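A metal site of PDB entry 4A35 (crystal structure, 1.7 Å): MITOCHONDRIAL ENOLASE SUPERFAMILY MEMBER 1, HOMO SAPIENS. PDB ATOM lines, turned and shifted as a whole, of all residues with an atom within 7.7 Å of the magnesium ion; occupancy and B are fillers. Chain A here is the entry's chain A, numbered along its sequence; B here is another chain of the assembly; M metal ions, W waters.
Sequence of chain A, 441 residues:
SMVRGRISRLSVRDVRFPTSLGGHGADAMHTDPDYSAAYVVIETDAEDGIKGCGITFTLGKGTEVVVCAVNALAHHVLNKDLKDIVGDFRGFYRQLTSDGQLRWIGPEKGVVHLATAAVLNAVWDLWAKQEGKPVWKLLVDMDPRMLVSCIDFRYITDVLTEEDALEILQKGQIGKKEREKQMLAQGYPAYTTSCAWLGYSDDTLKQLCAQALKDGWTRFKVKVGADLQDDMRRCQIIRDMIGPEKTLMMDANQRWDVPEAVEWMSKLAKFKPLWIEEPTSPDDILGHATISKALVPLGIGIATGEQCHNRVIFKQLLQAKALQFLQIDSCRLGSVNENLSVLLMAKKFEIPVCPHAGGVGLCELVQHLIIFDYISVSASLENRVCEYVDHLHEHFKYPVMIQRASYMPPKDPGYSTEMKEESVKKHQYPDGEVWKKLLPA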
ATOM      1  N   ASP A  27     -11.787 -25.989  20.434  1.00  0.00           N
ATOM      2  CA  ASP A  27     -12.057 -24.623  19.977  1.00  0.00           C
ATOM      3  C   ASP A  27     -12.310 -24.704  18.465  1.00  0.00           C
ATOM      4  O   ASP A  27     -12.337 -25.821  17.910  1.00  0.00           O
ATOM      5  CB  ASP A  27     -10.948 -23.620  20.396  1.00  0.00           C
ATOM      6  CG  ASP A  27      -9.578 -23.854  19.792  1.00  0.00           C
ATOM      7  OD1 ASP A  27      -9.479 -23.899  18.533  1.00  0.00           O
ATOM      8  OD2 ASP A  27      -8.627 -23.855  20.539  1.00  0.00           O
ATOM      9  N   TYR A 191     -10.488 -14.952  35.265  1.00  0.00           N
ATOM     10  CA  TYR A 191     -11.709 -15.246  34.527  1.00  0.00           C
ATOM     11  C   TYR A 191     -11.664 -16.716  34.248  1.00  0.00           C
ATOM     12  O   TYR A 191     -10.554 -17.306  34.215  1.00  0.00           O
ATOM     13  CB  TYR A 191     -11.822 -14.418  33.227  1.00  0.00           C
ATOM     14  CG  TYR A 191     -10.858 -14.756  32.112  1.00  0.00           C
ATOM     15  CD1 TYR A 191     -11.198 -15.684  31.124  1.00  0.00           C
ATOM     16  CD2 TYR A 191      -9.704 -13.995  31.908  1.00  0.00           C
ATOM     17  CE1 TYR A 191     -10.351 -15.943  30.046  1.00  0.00           C
ATOM     18  CE2 TYR A 191      -8.885 -14.181  30.771  1.00  0.00           C
ATOM     19  CZ  TYR A 191      -9.223 -15.160  29.848  1.00  0.00           C
ATOM     20  OH  TYR A 191      -8.424 -15.393  28.771  1.00  0.00           O
ATOM     21  N   THR A 193     -12.487 -20.026  31.670  1.00  0.00           N
ATOM     22  CA  THR A 193     -12.659 -20.501  30.284  1.00  0.00           C
ATOM     23  C   THR A 193     -13.430 -21.855  30.348  1.00  0.00           C
ATOM     24  O   THR A 193     -13.637 -22.499  29.328  1.00  0.00           O
ATOM     25  CB  THR A 193     -11.292 -20.527  29.582  1.00  0.00           C
ATOM     26  OG1 THR A 193     -10.852 -19.173  29.570  1.00  0.00           O
ATOM     27  CG2 THR A 193     -11.357 -21.017  28.077  1.00  0.00           C
ATOM     28  N   TRP A 197     -15.954 -23.927  25.722  1.00  0.00           N
ATOM     29  CA  TRP A 197     -15.633 -24.925  24.693  1.00  0.00           C
ATOM     30  C   TRP A 197     -16.760 -25.261  23.745  1.00  0.00           C
ATOM     31  O   TRP A 197     -17.945 -25.100  24.071  1.00  0.00           O
ATOM     32  CB  TRP A 197     -15.013 -26.194  25.326  1.00  0.00           C
ATOM     33  CG  TRP A 197     -13.950 -25.874  26.364  1.00  0.00           C
ATOM     34  CD1 TRP A 197     -14.034 -26.066  27.713  1.00  0.00           C
ATOM     35  CD2 TRP A 197     -12.665 -25.264  26.118  1.00  0.00           C
ATOM     36  NE1 TRP A 197     -12.844 -25.670  28.327  1.00  0.00           N
ATOM     37  CE2 TRP A 197     -12.008 -25.151  27.368  1.00  0.00           C
ATOM     38  CE3 TRP A 197     -11.982 -24.841  24.950  1.00  0.00           C
ATOM     39  CZ2 TRP A 197     -10.710 -24.596  27.494  1.00  0.00           C
ATOM     40  CZ3 TRP A 197     -10.674 -24.387  25.066  1.00  0.00           C
ATOM     41  CH2 TRP A 197     -10.068 -24.229  26.328  1.00  0.00           C
ATOM     42  N   LYS A 221     -15.056 -16.548  29.438  1.00  0.00           N
ATOM     43  CA  LYS A 221     -14.647 -16.570  28.048  1.00  0.00           C
ATOM     44  C   LYS A 221     -15.497 -17.577  27.310  1.00  0.00           C
ATOM     45  O   LYS A 221     -15.950 -18.573  27.889  1.00  0.00           O
ATOM     46  CB  LYS A 221     -13.132 -16.869  27.858  1.00  0.00           C
ATOM     47  CG  LYS A 221     -12.662 -16.587  26.430  1.00  0.00           C
ATOM     48  CD  LYS A 221     -11.225 -16.058  26.344  1.00  0.00           C
ATOM     49  CE  LYS A 221     -10.331 -17.246  26.326  1.00  0.00           C
ATOM     50  NZ  LYS A 221      -8.896 -16.841  26.402  1.00  0.00           N
ATOM     51  N   LYS A 223     -15.514 -19.585  23.292  1.00  0.00           N
ATOM     52  CA  LYS A 223     -14.888 -19.818  21.994  1.00  0.00           C
ATOM     53  C   LYS A 223     -15.911 -19.596  20.899  1.00  0.00           C
ATOM     54  O   LYS A 223     -17.073 -20.047  21.007  1.00  0.00           O
ATOM     55  CB  LYS A 223     -14.352 -21.265  21.875  1.00  0.00           C
ATOM     56  CG  LYS A 223     -13.289 -21.643  22.892  1.00  0.00           C
ATOM     57  CD  LYS A 223     -12.028 -20.752  22.756  1.00  0.00           C
ATOM     58  CE  LYS A 223     -11.204 -20.913  24.014  1.00  0.00           C
ATOM     59  NZ  LYS A 223      -9.761 -20.647  23.766  1.00  0.00           N
ATOM     60  N   MET A 250     -14.682 -13.122  24.067  1.00  0.00           N
ATOM     61  CA  MET A 250     -14.755 -14.091  22.935  1.00  0.00           C
ATOM     62  C   MET A 250     -13.357 -14.433  22.426  1.00  0.00           C
ATOM     63  O   MET A 250     -12.455 -13.562  22.434  1.00  0.00           O
ATOM     64  CB  MET A 250     -15.639 -13.526  21.816  1.00  0.00           C
ATOM     65  CG  MET A 250     -17.107 -13.380  22.258  1.00  0.00           C
ATOM     66  SD  MET A 250     -17.974 -12.478  20.973  1.00  0.00           S
ATOM     67  CE  MET A 250     -19.646 -12.307  21.689  1.00  0.00           C
ATOM     68  N   ASP A 251     -13.201 -15.653  21.874  1.00  0.00           N
ATOM     69  CA  ASP A 251     -11.896 -16.123  21.411  1.00  0.00           C
ATOM     70  C   ASP A 251     -12.095 -16.902  20.118  1.00  0.00           C
ATOM     71  O   ASP A 251     -12.783 -17.921  20.111  1.00  0.00           O
ATOM     72  CB  ASP A 251     -11.244 -16.996  22.519  1.00  0.00           C
ATOM     73  CG  ASP A 251      -9.823 -17.448  22.192  1.00  0.00           C
ATOM     74  OD1 ASP A 251      -9.381 -17.232  21.036  1.00  0.00           O
ATOM     75  OD2 ASP A 251      -9.170 -18.064  23.066  1.00  0.00           O
ATOM     76  N   ALA A 252     -11.588 -16.365  19.005  1.00  0.00           N
ATOM     77  CA  ALA A 252     -11.753 -16.970  17.671  1.00  0.00           C
ATOM     78  C   ALA A 252     -10.590 -17.896  17.317  1.00  0.00           C
ATOM     79  O   ALA A 252     -10.669 -18.485  16.236  1.00  0.00           O
ATOM     80  CB  ALA A 252     -11.894 -15.887  16.607  1.00  0.00           C
ATOM     81  N   ASN A 253      -9.523 -17.987  18.169  1.00  0.00           N
ATOM     82  CA  ASN A 253      -8.373 -18.899  17.868  1.00  0.00           C
ATOM     83  C   ASN A 253      -7.909 -18.833  16.386  1.00  0.00           C
ATOM     84  O   ASN A 253      -7.670 -19.895  15.728  1.00  0.00           O
ATOM     85  CB  ASN A 253      -8.770 -20.376  18.210  1.00  0.00           C
ATOM     86  CG  ASN A 253      -8.882 -20.576  19.705  1.00  0.00           C
ATOM     87  OD1 ASN A 253      -9.971 -20.480  20.263  1.00  0.00           O
ATOM     88  ND2 ASN A 253      -7.744 -20.642  20.396  1.00  0.00           N
ATOM     89  N   GLN A 254      -7.736 -17.560  15.875  1.00  0.00           N
ATOM     90  CA  GLN A 254      -7.102 -17.274  14.568  1.00  0.00           C
ATOM     91  C   GLN A 254      -7.935 -17.677  13.354  1.00  0.00           C
ATOM     92  O   GLN A 254      -7.406 -17.724  12.258  1.00  0.00           O
ATOM     93  CB  GLN A 254      -5.707 -17.997  14.454  1.00  0.00           C
ATOM     94  CG  GLN A 254      -4.853 -17.869  15.725  1.00  0.00           C
ATOM     95  CD  GLN A 254      -3.746 -18.915  15.824  1.00  0.00           C
ATOM     96  OE1 GLN A 254      -3.632 -19.826  14.993  1.00  0.00           O
ATOM     97  NE2 GLN A 254      -2.948 -18.843  16.891  1.00  0.00           N
ATOM     98  N   TRP A 275     -13.655  -8.192  24.813  1.00  0.00           N
ATOM     99  CA  TRP A 275     -12.655  -8.324  23.791  1.00  0.00           C
ATOM    100  C   TRP A 275     -12.955  -9.499  22.863  1.00  0.00           C
ATOM    101  O   TRP A 275     -13.733 -10.436  23.214  1.00  0.00           O
ATOM    102  CB  TRP A 275     -11.230  -8.489  24.376  1.00  0.00           C
ATOM    103  CG  TRP A 275     -10.861  -9.796  25.048  1.00  0.00           C
ATOM    104  CD1 TRP A 275     -10.773 -11.024  24.465  1.00  0.00           C
ATOM    105  CD2 TRP A 275     -10.251  -9.917  26.339  1.00  0.00           C
ATOM    106  NE1 TRP A 275     -10.269 -11.943  25.371  1.00  0.00           N
ATOM    107  CE2 TRP A 275      -9.918 -11.293  26.523  1.00  0.00           C
ATOM    108  CE3 TRP A 275      -9.976  -8.990  27.389  1.00  0.00           C
ATOM    109  CZ2 TRP A 275      -9.285 -11.765  27.686  1.00  0.00           C
ATOM    110  CZ3 TRP A 275      -9.380  -9.467  28.548  1.00  0.00           C
ATOM    111  CH2 TRP A 275      -9.015 -10.829  28.681  1.00  0.00           C
ATOM    112  N   GLU A 277     -10.542 -12.192  21.056  1.00  0.00           N
ATOM    113  CA  GLU A 277      -9.189 -12.708  21.163  1.00  0.00           C
ATOM    114  C   GLU A 277      -8.817 -13.480  19.863  1.00  0.00           C
ATOM    115  O   GLU A 277      -9.615 -14.259  19.335  1.00  0.00           O
ATOM    116  CB  GLU A 277      -9.110 -13.595  22.407  1.00  0.00           C
ATOM    117  CG  GLU A 277      -7.773 -14.306  22.608  1.00  0.00           C
ATOM    118  CD  GLU A 277      -7.778 -15.054  23.945  1.00  0.00           C
ATOM    119  OE1 GLU A 277      -8.516 -14.601  24.850  1.00  0.00           O
ATOM    120  OE2 GLU A 277      -6.957 -15.989  24.138  1.00  0.00           O
ATOM    121  N   GLU A 278      -7.540 -13.308  19.408  1.00  0.00           N
ATOM    122  CA  GLU A 278      -6.977 -13.925  18.221  1.00  0.00           C
ATOM    123  C   GLU A 278      -7.973 -13.917  17.034  1.00  0.00           C
ATOM    124  O   GLU A 278      -8.308 -14.991  16.498  1.00  0.00           O
ATOM    125  CB  GLU A 278      -6.509 -15.352  18.514  1.00  0.00           C
ATOM    126  CG  GLU A 278      -5.302 -15.397  19.432  1.00  0.00           C
ATOM    127  CD  GLU A 278      -4.515 -16.643  19.127  1.00  0.00           C
ATOM    128  OE1 GLU A 278      -5.021 -17.760  19.448  1.00  0.00           O
ATOM    129  OE2 GLU A 278      -3.398 -16.528  18.563  1.00  0.00           O
ATOM    130  N   ALA A 303      -7.691  -8.576  21.637  1.00  0.00           N
ATOM    131  CA  ALA A 303      -6.720  -9.277  22.498  1.00  0.00           C
ATOM    132  C   ALA A 303      -5.925 -10.283  21.641  1.00  0.00           C
ATOM    133  O   ALA A 303      -6.517 -10.983  20.819  1.00  0.00           O
ATOM    134  CB  ALA A 303      -7.440 -10.037  23.632  1.00  0.00           C
ATOM    135  N   THR A 304      -4.619 -10.392  21.858  1.00  0.00           N
ATOM    136  CA  THR A 304      -3.891 -11.454  21.163  1.00  0.00           C
ATOM    137  C   THR A 304      -2.601 -11.708  21.905  1.00  0.00           C
ATOM    138  O   THR A 304      -2.215 -10.899  22.770  1.00  0.00           O
ATOM    139  CB  THR A 304      -3.653 -11.160  19.621  1.00  0.00           C
ATOM    140  OG1 THR A 304      -3.108 -12.366  19.014  1.00  0.00           O
ATOM    141  CG2 THR A 304      -2.646  -9.993  19.392  1.00  0.00           C
ATOM    142  N   GLY A 305      -1.956 -12.819  21.555  1.00  0.00           N
ATOM    143  CA  GLY A 305      -0.640 -13.098  22.098  1.00  0.00           C
ATOM    144  C   GLY A 305      -0.295 -14.506  22.498  1.00  0.00           C
ATOM    145  O   GLY A 305       0.899 -14.808  22.588  1.00  0.00           O
ATOM    146  N   GLU A 306      -1.290 -15.362  22.816  1.00  0.00           N
ATOM    147  CA  GLU A 306      -0.929 -16.702  23.297  1.00  0.00           C
ATOM    148  C   GLU A 306      -0.018 -17.501  22.324  1.00  0.00           C
ATOM    149  O   GLU A 306       0.747 -18.311  22.828  1.00  0.00           O
ATOM    150  CB  GLU A 306      -2.176 -17.546  23.590  1.00  0.00           C
ATOM    151  CG  GLU A 306      -2.872 -18.063  22.353  1.00  0.00           C
ATOM    152  CD  GLU A 306      -4.152 -18.763  22.728  1.00  0.00           C
ATOM    153  OE1 GLU A 306      -4.957 -18.132  23.443  1.00  0.00           O
ATOM    154  OE2 GLU A 306      -4.323 -19.942  22.363  1.00  0.00           O
ATOM    155  N   GLN A 307      -0.092 -17.287  20.949  1.00  0.00           N
ATOM    156  CA  GLN A 307       0.767 -18.005  20.015  1.00  0.00           C
ATOM    157  C   GLN A 307       1.767 -17.043  19.382  1.00  0.00           C
ATOM    158  O   GLN A 307       2.450 -17.422  18.422  1.00  0.00           O
ATOM    159  CB  GLN A 307      -0.078 -18.740  18.931  1.00  0.00           C
ATOM    160  CG  GLN A 307      -0.824 -19.958  19.516  1.00  0.00           C
ATOM    161  CD  GLN A 307      -0.921 -21.130  18.548  1.00  0.00           C
ATOM    162  OE1 GLN A 307      -2.020 -21.534  18.127  1.00  0.00           O
ATOM    163  NE2 GLN A 307       0.193 -21.801  18.295  1.00  0.00           N
ATOM    164  N   GLN A 327      -1.702 -10.584  25.572  1.00  0.00           N
ATOM    165  CA  GLN A 327      -1.747 -11.858  26.279  1.00  0.00           C
ATOM    166  C   GLN A 327      -0.410 -12.585  26.234  1.00  0.00           C
ATOM    167  O   GLN A 327      -0.146 -13.326  25.300  1.00  0.00           O
ATOM    168  CB  GLN A 327      -2.882 -12.722  25.690  1.00  0.00           C
ATOM    169  CG  GLN A 327      -4.193 -11.888  25.814  1.00  0.00           C
ATOM    170  CD  GLN A 327      -5.352 -12.483  25.138  1.00  0.00           C
ATOM    171  OE1 GLN A 327      -5.306 -12.743  23.931  1.00  0.00           O
ATOM    172  NE2 GLN A 327      -6.419 -12.674  25.909  1.00  0.00           N
ATOM    173  N   HIS A 356      -2.462 -15.515  29.046  1.00  0.00           N
ATOM    174  CA  HIS A 356      -3.075 -16.731  28.586  1.00  0.00           C
ATOM    175  C   HIS A 356      -2.704 -17.823  29.606  1.00  0.00           C
ATOM    176  O   HIS A 356      -1.591 -17.845  30.149  1.00  0.00           O
ATOM    177  CB  HIS A 356      -2.599 -17.111  27.156  1.00  0.00           C
ATOM    178  CG  HIS A 356      -2.905 -18.520  26.732  1.00  0.00           C
ATOM    179  ND1 HIS A 356      -1.913 -19.515  26.713  1.00  0.00           N
ATOM    180  CD2 HIS A 356      -4.061 -19.059  26.309  1.00  0.00           C
ATOM    181  CE1 HIS A 356      -2.512 -20.613  26.269  1.00  0.00           C
ATOM    182  NE2 HIS A 356      -3.799 -20.396  25.994  1.00  0.00           N
ATOM    183  N   ALA A 357      -3.599 -18.764  29.795  1.00  0.00           N
ATOM    184  CA  ALA A 357      -3.302 -19.881  30.689  1.00  0.00           C
ATOM    185  C   ALA A 357      -4.166 -21.120  30.305  1.00  0.00           C
ATOM    186  O   ALA A 357      -4.572 -21.232  29.133  1.00  0.00           O
ATOM    187  CB  ALA A 357      -3.499 -19.456  32.143  1.00  0.00           C
ATOM    188  N   GLU A 387      -6.222 -15.485  32.859  1.00  0.00           N
ATOM    189  CA  GLU A 387      -7.086 -16.604  32.494  1.00  0.00           C
ATOM    190  C   GLU A 387      -6.965 -17.759  33.513  1.00  0.00           C
ATOM    191  O   GLU A 387      -5.893 -17.993  34.077  1.00  0.00           O
ATOM    192  CB  GLU A 387      -6.733 -17.107  31.100  1.00  0.00           C
ATOM    193  CG  GLU A 387      -7.603 -18.242  30.560  1.00  0.00           C
ATOM    194  CD  GLU A 387      -7.414 -18.489  29.069  1.00  0.00           C
ATOM    195  OE1 GLU A 387      -6.289 -18.270  28.555  1.00  0.00           O
ATOM    196  OE2 GLU A 387      -8.398 -18.923  28.416  1.00  0.00           O
ATOM    197  N   TRP B 104       0.054 -26.399  16.572  1.00  0.00           N
ATOM    198  CA  TRP B 104       0.425 -25.715  17.820  1.00  0.00           C
ATOM    199  C   TRP B 104       1.945 -25.535  17.904  1.00  0.00           C
ATOM    200  O   TRP B 104       2.412 -24.566  18.505  1.00  0.00           O
ATOM    201  CB  TRP B 104      -0.028 -26.538  19.043  1.00  0.00           C
ATOM    202  CG  TRP B 104       0.071 -25.779  20.342  1.00  0.00           C
ATOM    203  CD1 TRP B 104       1.081 -25.863  21.264  1.00  0.00           C
ATOM    204  CD2 TRP B 104      -0.868 -24.840  20.857  1.00  0.00           C
ATOM    205  NE1 TRP B 104       0.834 -25.007  22.308  1.00  0.00           N
ATOM    206  CE2 TRP B 104      -0.376 -24.394  22.116  1.00  0.00           C
ATOM    207  CE3 TRP B 104      -2.095 -24.327  20.386  1.00  0.00           C
ATOM    208  CZ2 TRP B 104      -1.020 -23.388  22.852  1.00  0.00           C
ATOM    209  CZ3 TRP B 104      -2.770 -23.384  21.158  1.00  0.00           C
ATOM    210  CH2 TRP B 104      -2.248 -22.958  22.390  1.00  0.00           C
HETATM  211 MG    MG M   1      -7.020 -18.015  23.353  1.00  0.00          MG
HETATM  212  O   HOH W   1      -6.874 -20.401  22.997  1.00  0.00           O
HETATM  213  O   HOH W   2      -6.898 -17.755  21.428  1.00  0.00           O
HETATM  214  O   HOH W   3      -7.165 -18.887  25.100  1.00  0.00           O
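NZ of Lys 221 touches the magnesium ion, at 3.8 Å. Lys 223 touches the magnesium ion.
The magnesium ion is bound by water W2 (1.9 Å), water W3 (2.0 Å), the side-chain carboxylate (OE1) of Glu 306 (2.1 Å), the side-chain carboxylate (OD2) of Asp 251 (2.2 Å), the side-chain carboxylate (OE2) of Glu 277 (2.2 Å) and water W1 (2.4 Å).
The backbone carbonyl oxygen (O) of Gln 327 is in hydrogen-bond range of the backbone NH (N) of Glu 306. NZ of Lys 221 lies close to OD2 of Asp 251 (3.6 Å). The side-chain carboxylate (OD2) of Asp 251 sits close to the side-chain amino group (NZ) of Lys 223. N of Asn 253 lies within hydrogen-bond range of OD1 of Asp 251. OE1 of Glu 277 is in salt-bridge range of NZ of Lys 221 (2.8 Å). The backbone NH (N) of Ala 252 sits at hydrogen-bond distance from the backbone carbonyl oxygen (O) of Glu 277, at 2.9 Å. N of Glu 277 is in hydrogen-bond range of O of Met 250 (2.7 Å). The side-chain hydroxyl (OH) of Tyr 191 is in hydrogen-bond range of the side-chain amino group (NZ) of Lys 221, at 2.8 Å.
Water W1 lies within hydrogen-bond range of the side-chain carboxylate of Glu 306 (2.7 Å), the side-chain amide nitrogen of Asn 253 (2.8 Å) and the side-chain amino group of Lys 223 (3.0 Å). Water W3 lies within hydrogen-bond range of NZ of Lys 221 and NZ of Lys 223. Water W2 lies within hydrogen-bond range of OD1 of Asp 251, OE1 of Glu 278 and ND2 of Asn 253.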
